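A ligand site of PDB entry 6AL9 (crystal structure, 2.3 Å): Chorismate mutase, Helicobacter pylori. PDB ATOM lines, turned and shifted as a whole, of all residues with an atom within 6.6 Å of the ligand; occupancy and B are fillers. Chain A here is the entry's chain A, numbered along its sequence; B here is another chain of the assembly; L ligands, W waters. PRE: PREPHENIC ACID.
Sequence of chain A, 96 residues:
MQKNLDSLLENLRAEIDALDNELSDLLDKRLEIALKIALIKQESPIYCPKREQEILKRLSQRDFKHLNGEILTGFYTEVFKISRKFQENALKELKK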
ATOM      1  N   ARG A  30     -18.575 -31.668  33.286  1.00  0.00           N
ATOM      2  CA  ARG A  30     -18.474 -30.852  32.083  1.00  0.00           C
ATOM      3  C   ARG A  30     -19.645 -31.125  31.157  1.00  0.00           C
ATOM      4  O   ARG A  30     -20.101 -30.205  30.438  1.00  0.00           O
ATOM      5  CB  ARG A  30     -17.144 -31.103  31.380  1.00  0.00           C
ATOM      6  CG  ARG A  30     -16.800 -30.098  30.289  1.00  0.00           C
ATOM      7  CD  ARG A  30     -15.688 -30.632  29.411  1.00  0.00           C
ATOM      8  NE  ARG A  30     -15.043 -29.588  28.631  1.00  0.00           N
ATOM      9  CZ  ARG A  30     -15.509 -29.115  27.477  1.00  0.00           C
ATOM     10  NH1 ARG A  30     -16.646 -29.589  26.939  1.00  0.00           N
ATOM     11  NH2 ARG A  30     -14.847 -28.155  26.854  1.00  0.00           N
ATOM     12  N   ALA A  34     -22.559 -28.454  29.988  1.00  0.00           N
ATOM     13  CA  ALA A  34     -23.017 -28.416  28.589  1.00  0.00           C
ATOM     14  C   ALA A  34     -24.519 -28.669  28.462  1.00  0.00           C
ATOM     15  O   ALA A  34     -25.162 -28.197  27.522  1.00  0.00           O
ATOM     16  CB  ALA A  34     -22.219 -29.382  27.710  1.00  0.00           C
ATOM     17  N   ILE A  37     -26.035 -25.370  29.160  1.00  0.00           N
ATOM     18  CA  ILE A  37     -25.842 -24.527  28.005  1.00  0.00           C
ATOM     19  C   ILE A  37     -26.855 -24.897  26.925  1.00  0.00           C
ATOM     20  O   ILE A  37     -27.450 -24.024  26.315  1.00  0.00           O
ATOM     21  CB  ILE A  37     -24.410 -24.638  27.436  1.00  0.00           C
ATOM     22  CG1 ILE A  37     -23.405 -23.950  28.361  1.00  0.00           C
ATOM     23  CG2 ILE A  37     -24.334 -23.986  26.070  1.00  0.00           C
ATOM     24  CD1 ILE A  37     -21.947 -24.246  28.070  1.00  0.00           C
ATOM     25  N   ALA A  38     -27.052 -26.185  26.655  1.00  0.00           N
ATOM     26  CA  ALA A  38     -28.022 -26.603  25.646  1.00  0.00           C
ATOM     27  C   ALA A  38     -29.368 -26.015  25.961  1.00  0.00           C
ATOM     28  O   ALA A  38     -30.064 -25.576  25.065  1.00  0.00           O
ATOM     29  CB  ALA A  38     -28.138 -28.114  25.606  1.00  0.00           C
ATOM     30  N   LYS A  41     -29.962 -22.341  25.364  1.00  0.00           N
ATOM     31  CA  LYS A  41     -29.742 -21.940  23.988  1.00  0.00           C
ATOM     32  C   LYS A  41     -30.478 -22.769  22.964  1.00  0.00           C
ATOM     33  O   LYS A  41     -29.898 -23.097  21.928  1.00  0.00           O
ATOM     34  CB  LYS A  41     -28.250 -21.986  23.687  1.00  0.00           C
ATOM     35  CG  LYS A  41     -27.567 -20.746  24.175  1.00  0.00           C
ATOM     36  CD  LYS A  41     -27.892 -19.586  23.245  1.00  0.00           C
ATOM     37  CE  LYS A  41     -26.895 -19.569  22.103  1.00  0.00           C
ATOM     38  NZ  LYS A  41     -25.616 -18.989  22.606  1.00  0.00           N
ATOM     39  N   PRO A  45     -27.717 -23.331  16.879  1.00  0.00           N
ATOM     40  CA  PRO A  45     -26.954 -24.530  16.571  1.00  0.00           C
ATOM     41  C   PRO A  45     -26.052 -24.948  17.718  1.00  0.00           C
ATOM     42  O   PRO A  45     -25.496 -24.075  18.406  1.00  0.00           O
ATOM     43  CB  PRO A  45     -26.078 -24.094  15.392  1.00  0.00           C
ATOM     44  CG  PRO A  45     -25.956 -22.604  15.529  1.00  0.00           C
ATOM     45  CD  PRO A  45     -27.256 -22.166  16.117  1.00  0.00           C
ATOM     46  N   ILE A  46     -25.877 -26.259  17.919  1.00  0.00           N
ATOM     47  CA  ILE A  46     -24.957 -26.746  18.953  1.00  0.00           C
ATOM     48  C   ILE A  46     -23.501 -26.517  18.572  1.00  0.00           C
ATOM     49  O   ILE A  46     -22.735 -25.980  19.365  1.00  0.00           O
ATOM     50  CB  ILE A  46     -25.205 -28.204  19.276  1.00  0.00           C
ATOM     51  CG1 ILE A  46     -26.506 -28.342  20.060  1.00  0.00           C
ATOM     52  CG2 ILE A  46     -24.054 -28.753  20.090  1.00  0.00           C
ATOM     53  CD1 ILE A  46     -26.903 -29.767  20.358  1.00  0.00           C
ATOM     54  N   TYR A  47     -23.130 -26.877  17.347  1.00  0.00           N
ATOM     55  CA  TYR A  47     -21.741 -26.758  16.914  1.00  0.00           C
ATOM     56  C   TYR A  47     -21.345 -25.263  16.879  1.00  0.00           C
ATOM     57  O   TYR A  47     -21.872 -24.508  16.080  1.00  0.00           O
ATOM     58  CB  TYR A  47     -21.571 -27.425  15.554  1.00  0.00           C
ATOM     59  CG  TYR A  47     -20.155 -27.532  15.019  1.00  0.00           C
ATOM     60  CD1 TYR A  47     -19.065 -27.793  15.856  1.00  0.00           C
ATOM     61  CD2 TYR A  47     -19.915 -27.387  13.652  1.00  0.00           C
ATOM     62  CE1 TYR A  47     -17.781 -27.890  15.336  1.00  0.00           C
ATOM     63  CE2 TYR A  47     -18.653 -27.492  13.141  1.00  0.00           C
ATOM     64  CZ  TYR A  47     -17.595 -27.739  13.970  1.00  0.00           C
ATOM     65  OH  TYR A  47     -16.349 -27.835  13.417  1.00  0.00           O
ATOM     66  N   CYS A  48     -20.450 -24.861  17.791  1.00  0.00           N
ATOM     67  CA  CYS A  48     -19.808 -23.551  17.756  1.00  0.00           C
ATOM     68  C   CYS A  48     -18.292 -23.660  17.545  1.00  0.00           C
ATOM     69  O   CYS A  48     -17.510 -23.704  18.501  1.00  0.00           O
ATOM     70  CB  CYS A  48     -20.133 -22.738  19.012  1.00  0.00           C
ATOM     71  SG  CYS A  48     -19.748 -20.956  18.853  1.00  0.00           S
ATOM     72  N   PRO A  49     -17.876 -23.754  16.283  1.00  0.00           N
ATOM     73  CA  PRO A  49     -16.462 -23.904  15.930  1.00  0.00           C
ATOM     74  C   PRO A  49     -15.519 -22.778  16.419  1.00  0.00           C
ATOM     75  O   PRO A  49     -14.378 -23.068  16.835  1.00  0.00           O
ATOM     76  CB  PRO A  49     -16.488 -23.993  14.399  1.00  0.00           C
ATOM     77  CG  PRO A  49     -17.900 -23.695  13.972  1.00  0.00           C
ATOM     78  CD  PRO A  49     -18.764 -24.038  15.143  1.00  0.00           C
ATOM     79  N   ARG A  51     -15.849 -21.051  19.272  1.00  0.00           N
ATOM     80  CA  ARG A  51     -15.625 -21.436  20.675  1.00  0.00           C
ATOM     81  C   ARG A  51     -14.654 -22.631  20.827  1.00  0.00           C
ATOM     82  O   ARG A  51     -13.759 -22.586  21.675  1.00  0.00           O
ATOM     83  CB  ARG A  51     -16.977 -21.751  21.357  1.00  0.00           C
ATOM     84  CG  ARG A  51     -16.927 -22.332  22.765  1.00  0.00           C
ATOM     85  CD  ARG A  51     -16.425 -21.340  23.807  1.00  0.00           C
ATOM     86  NE  ARG A  51     -16.397 -21.923  25.148  1.00  0.00           N
ATOM     87  CZ  ARG A  51     -15.610 -21.545  26.152  1.00  0.00           C
ATOM     88  NH1 ARG A  51     -14.755 -20.548  26.008  1.00  0.00           N
ATOM     89  NH2 ARG A  51     -15.680 -22.166  27.316  1.00  0.00           N
ATOM     90  N   GLU A  52     -14.829 -23.692  20.032  1.00  0.00           N
ATOM     91  CA  GLU A  52     -13.936 -24.862  20.107  1.00  0.00           C
ATOM     92  C   GLU A  52     -12.494 -24.437  19.858  1.00  0.00           C
ATOM     93  O   GLU A  52     -11.577 -24.911  20.548  1.00  0.00           O
ATOM     94  CB  GLU A  52     -14.332 -25.962  19.121  1.00  0.00           C
ATOM     95  CG  GLU A  52     -15.642 -26.662  19.479  1.00  0.00           C
ATOM     96  CD  GLU A  52     -15.968 -27.845  18.575  1.00  0.00           C
ATOM     97  OE1 GLU A  52     -15.108 -28.174  17.721  1.00  0.00           O
ATOM     98  OE2 GLU A  52     -17.067 -28.451  18.713  1.00  0.00           O
ATOM     99  N   ILE A  55     -11.150 -22.368  22.830  1.00  0.00           N
ATOM    100  CA  ILE A  55     -10.732 -23.302  23.893  1.00  0.00           C
ATOM    101  C   ILE A  55      -9.331 -23.872  23.638  1.00  0.00           C
ATOM    102  O   ILE A  55      -8.436 -23.740  24.475  1.00  0.00           O
ATOM    103  CB  ILE A  55     -11.777 -24.434  24.063  1.00  0.00           C
ATOM    104  CG1 ILE A  55     -13.014 -23.840  24.770  1.00  0.00           C
ATOM    105  CG2 ILE A  55     -11.193 -25.598  24.851  1.00  0.00           C
ATOM    106  CD1 ILE A  55     -14.137 -24.829  24.990  1.00  0.00           C
ATOM    107  N   VAL A  79     -13.542 -34.963  23.246  1.00  0.00           N
ATOM    108  CA  VAL A  79     -14.338 -34.226  24.246  1.00  0.00           C
ATOM    109  C   VAL A  79     -15.471 -33.393  23.609  1.00  0.00           C
ATOM    110  O   VAL A  79     -16.606 -33.439  24.104  1.00  0.00           O
ATOM    111  CB  VAL A  79     -13.452 -33.293  25.091  1.00  0.00           C
ATOM    112  CG1 VAL A  79     -14.304 -32.393  25.983  1.00  0.00           C
ATOM    113  CG2 VAL A  79     -12.525 -34.108  25.964  1.00  0.00           C
ATOM    114  N   PHE A  80     -15.176 -32.647  22.544  1.00  0.00           N
ATOM    115  CA  PHE A  80     -16.205 -31.883  21.831  1.00  0.00           C
ATOM    116  C   PHE A  80     -17.222 -32.787  21.119  1.00  0.00           C
ATOM    117  O   PHE A  80     -18.401 -32.503  21.124  1.00  0.00           O
ATOM    118  CB  PHE A  80     -15.623 -30.893  20.817  1.00  0.00           C
ATOM    119  CG  PHE A  80     -14.744 -29.826  21.405  1.00  0.00           C
ATOM    120  CD1 PHE A  80     -15.049 -29.220  22.599  1.00  0.00           C
ATOM    121  CD2 PHE A  80     -13.590 -29.417  20.726  1.00  0.00           C
ATOM    122  CE1 PHE A  80     -14.213 -28.255  23.110  1.00  0.00           C
ATOM    123  CE2 PHE A  80     -12.757 -28.443  21.225  1.00  0.00           C
ATOM    124  CZ  PHE A  80     -13.062 -27.866  22.417  1.00  0.00           C
ATOM    125  N   LYS A  81     -16.776 -33.876  20.512  1.00  0.00           N
ATOM    126  CA  LYS A  81     -17.695 -34.877  19.972  1.00  0.00           C
ATOM    127  C   LYS A  81     -18.629 -35.460  21.027  1.00  0.00           C
ATOM    128  O   LYS A  81     -19.846 -35.545  20.828  1.00  0.00           O
ATOM    129  CB  LYS A  81     -16.932 -36.012  19.319  1.00  0.00           C
ATOM    130  CG  LYS A  81     -16.489 -35.696  17.914  1.00  0.00           C
ATOM    131  CD  LYS A  81     -16.002 -36.930  17.176  1.00  0.00           C
ATOM    132  CE  LYS A  81     -15.267 -36.525  15.898  1.00  0.00           C
ATOM    133  NZ  LYS A  81     -14.205 -37.508  15.565  1.00  0.00           N
ATOM    134  N   SER A  83     -19.408 -34.087  23.901  1.00  0.00           N
ATOM    135  CA  SER A  83     -20.223 -32.990  24.398  1.00  0.00           C
ATOM    136  C   SER A  83     -21.335 -32.620  23.439  1.00  0.00           C
ATOM    137  O   SER A  83     -22.458 -32.334  23.865  1.00  0.00           O
ATOM    138  CB  SER A  83     -19.330 -31.751  24.617  1.00  0.00           C
ATOM    139  OG  SER A  83     -20.049 -30.644  25.097  1.00  0.00           O
ATOM    140  N   ARG A  84     -21.018 -32.635  22.144  1.00  0.00           N
ATOM    141  CA  ARG A  84     -21.992 -32.319  21.102  1.00  0.00           C
ATOM    142  C   ARG A  84     -23.110 -33.334  21.029  1.00  0.00           C
ATOM    143  O   ARG A  84     -24.278 -32.953  21.055  1.00  0.00           O
ATOM    144  CB  ARG A  84     -21.300 -32.234  19.734  1.00  0.00           C
ATOM    145  CG  ARG A  84     -21.310 -30.846  19.155  1.00  0.00           C
ATOM    146  CD  ARG A  84     -20.651 -30.791  17.792  1.00  0.00           C
ATOM    147  NE  ARG A  84     -19.222 -30.539  17.912  1.00  0.00           N
ATOM    148  CZ  ARG A  84     -18.273 -31.297  17.387  1.00  0.00           C
ATOM    149  NH1 ARG A  84     -18.565 -32.383  16.693  1.00  0.00           N
ATOM    150  NH2 ARG A  84     -17.002 -30.960  17.554  1.00  0.00           N
ATOM    151  N   GLN A  87     -25.373 -33.202  24.155  1.00  0.00           N
ATOM    152  CA  GLN A  87     -26.296 -32.070  24.096  1.00  0.00           C
ATOM    153  C   GLN A  87     -27.473 -32.327  23.147  1.00  0.00           C
ATOM    154  O   GLN A  87     -28.634 -32.086  23.506  1.00  0.00           O
ATOM    155  CB  GLN A  87     -25.587 -30.788  23.634  1.00  0.00           C
ATOM    156  CG  GLN A  87     -24.771 -30.073  24.698  1.00  0.00           C
ATOM    157  CD  GLN A  87     -24.018 -28.887  24.122  1.00  0.00           C
ATOM    158  OE1 GLN A  87     -22.801 -28.916  23.967  1.00  0.00           O
ATOM    159  NE2 GLN A  87     -24.753 -27.856  23.784  1.00  0.00           N
ATOM    160  N   LEU B   9     -24.721 -17.468  29.773  1.00  0.00           N
ATOM    161  CA  LEU B   9     -23.759 -18.190  28.978  1.00  0.00           C
ATOM    162  C   LEU B   9     -22.311 -17.888  29.366  1.00  0.00           C
ATOM    163  O   LEU B   9     -21.505 -18.804  29.448  1.00  0.00           O
ATOM    164  CB  LEU B   9     -24.003 -17.877  27.503  1.00  0.00           C
ATOM    165  CG  LEU B   9     -23.280 -18.749  26.472  1.00  0.00           C
ATOM    166  CD1 LEU B   9     -23.236 -20.228  26.872  1.00  0.00           C
ATOM    167  CD2 LEU B   9     -23.994 -18.580  25.143  1.00  0.00           C
ATOM    168  N   ARG B  13     -19.685 -20.816  30.650  1.00  0.00           N
ATOM    169  CA  ARG B  13     -18.500 -21.020  29.842  1.00  0.00           C
ATOM    170  C   ARG B  13     -17.234 -20.812  30.628  1.00  0.00           C
ATOM    171  O   ARG B  13     -16.219 -21.438  30.337  1.00  0.00           O
ATOM    172  CB  ARG B  13     -18.517 -20.093  28.642  1.00  0.00           C
ATOM    173  CG  ARG B  13     -19.356 -20.639  27.507  1.00  0.00           C
ATOM    174  CD  ARG B  13     -19.263 -19.736  26.288  1.00  0.00           C
ATOM    175  NE  ARG B  13     -19.515 -20.474  25.068  1.00  0.00           N
ATOM    176  CZ  ARG B  13     -19.962 -19.918  23.940  1.00  0.00           C
ATOM    177  NH1 ARG B  13     -20.193 -20.659  22.862  1.00  0.00           N
ATOM    178  NH2 ARG B  13     -20.228 -18.623  23.903  1.00  0.00           N
ATOM    179  N   ILE B  16     -16.982 -24.312  32.391  1.00  0.00           N
ATOM    180  CA  ILE B  16     -16.286 -25.143  31.378  1.00  0.00           C
ATOM    181  C   ILE B  16     -14.767 -24.876  31.351  1.00  0.00           C
ATOM    182  O   ILE B  16     -13.979 -25.799  31.407  1.00  0.00           O
ATOM    183  CB  ILE B  16     -16.828 -24.850  29.967  1.00  0.00           C
ATOM    184  CG1 ILE B  16     -18.278 -25.329  29.844  1.00  0.00           C
ATOM    185  CG2 ILE B  16     -15.935 -25.422  28.881  1.00  0.00           C
ATOM    186  CD1 ILE B  16     -18.500 -26.813  29.789  1.00  0.00           C
ATOM    187  N   ASP B  20     -11.759 -27.334  32.017  1.00  0.00           N
ATOM    188  CA  ASP B  20     -10.758 -27.642  31.034  1.00  0.00           C
ATOM    189  C   ASP B  20      -9.337 -27.420  31.523  1.00  0.00           C
ATOM    190  O   ASP B  20      -8.471 -28.178  31.152  1.00  0.00           O
ATOM    191  CB  ASP B  20     -11.014 -26.863  29.748  1.00  0.00           C
ATOM    192  CG  ASP B  20     -12.197 -27.417  28.972  1.00  0.00           C
ATOM    193  OD1 ASP B  20     -12.524 -28.611  29.157  1.00  0.00           O
ATOM    194  OD2 ASP B  20     -12.800 -26.670  28.153  1.00  0.00           O
HETATM  195  C1  PRE L   1     -19.150 -26.934  23.629  1.00  0.00           C
HETATM  196  C2  PRE L   1     -20.008 -27.917  22.900  1.00  0.00           C
HETATM  197  C3  PRE L   1     -20.319 -27.778  21.612  1.00  0.00           C
HETATM  198  C4  PRE L   1     -19.866 -26.606  20.769  1.00  0.00           C
HETATM  199  O4  PRE L   1     -19.213 -27.083  19.583  1.00  0.00           O
HETATM  200  C5  PRE L   1     -18.951 -25.664  21.508  1.00  0.00           C
HETATM  201  C6  PRE L   1     -18.645 -25.797  22.801  1.00  0.00           C
HETATM  202  C7  PRE L   1     -18.049 -27.621  24.386  1.00  0.00           C
HETATM  203  O71 PRE L   1     -18.030 -28.862  24.465  1.00  0.00           O
HETATM  204  O72 PRE L   1     -17.211 -26.909  24.957  1.00  0.00           O
HETATM  205  C8  PRE L   1     -20.067 -26.319  24.699  1.00  0.00           C
HETATM  206  C1' PRE L   1     -21.041 -25.342  24.086  1.00  0.00           C
HETATM  207  O1' PRE L   1     -22.091 -25.726  23.606  1.00  0.00           O
HETATM  208  C2' PRE L   1     -20.738 -23.912  24.046  1.00  0.00           C
HETATM  209  O'L PRE L   1     -21.440 -23.188  23.307  1.00  0.00           O
HETATM  210  O'M PRE L   1     -19.807 -23.456  24.740  1.00  0.00           O
HETATM  211  O   HOH W   1     -17.737 -24.066  25.976  1.00  0.00           O
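An oxygen (O4) of the ligand is in hydrogen-bond range of the side-chain carboxylate (OE2) of Glu 52, 2.7 Å away.
An oxygen (O71) of the ligand sits at hydrogen-bond distance from the side-chain hydroxyl of Ser 83 (2.8 Å).
NH1 of Arg 13 of chain B is in salt-bridge range of O'L of the ligand (2.9 Å).
The guanidinium group (NH1) of Arg 30 lies within salt-bridge range of an oxygen (O71) of the ligand (2.9 Å).
N of Cys 48 is in hydrogen-bond range of O4 of the ligand, 3.1 Å away.
An oxygen (O1') of the ligand lies close to the side-chain amide oxygen (OE1) of Gln 87, 3.3 Å away.
The guanidinium group (NE) of Arg 51 is in salt-bridge range of an oxygen (O'M) of the ligand, at 3.8 Å.
The side-chain carboxylate of Glu 52 lies within salt-bridge range of the guanidinium group of Arg 84, 2.8 Å away.
OE1 of Gln 87 sits close to O of Ser 83, at 3.4 Å.
The guanidinium group (NH2) of Arg 51 lies within hydrogen-bond range of the backbone carbonyl oxygen (O) of Arg 13 of chain B, 3.2 Å away.
OD1 of Asp 20 of chain B is in salt-bridge range of NE of Arg 30 (2.8 Å).
Ile 37 touches the ligand.
Ile 46 touches the ligand.
CA of Tyr 47 touches O4 of the ligand, at 3.7 Å.
Ile 55 touches the ligand (CD1 to O72, 3.7 Å).
Phe 80 touches the ligand.
Arg 84 touches the ligand.
Hydrophobic or aromatic side chains within 4 Å of the ligand: Ile 37, Tyr 47, Ile 55 and Phe 80.
13 residues have an atom within 4 Å of the ligand: Arg 30, Ile 37, Ile 46, Tyr 47, Cys 48, Arg 51, Glu 52, Ile 55, Phe 80, Ser 83, Arg 84, Gln 87 and Arg 13 of chain B.
The nearest printed residue that does not touch the ligand is Ile 16 of chain B (4.4 Å).
Water W1 lies within hydrogen-bond range of O'M of the ligand (2.5 Å) and NE of Arg 51 (2.7 Å).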
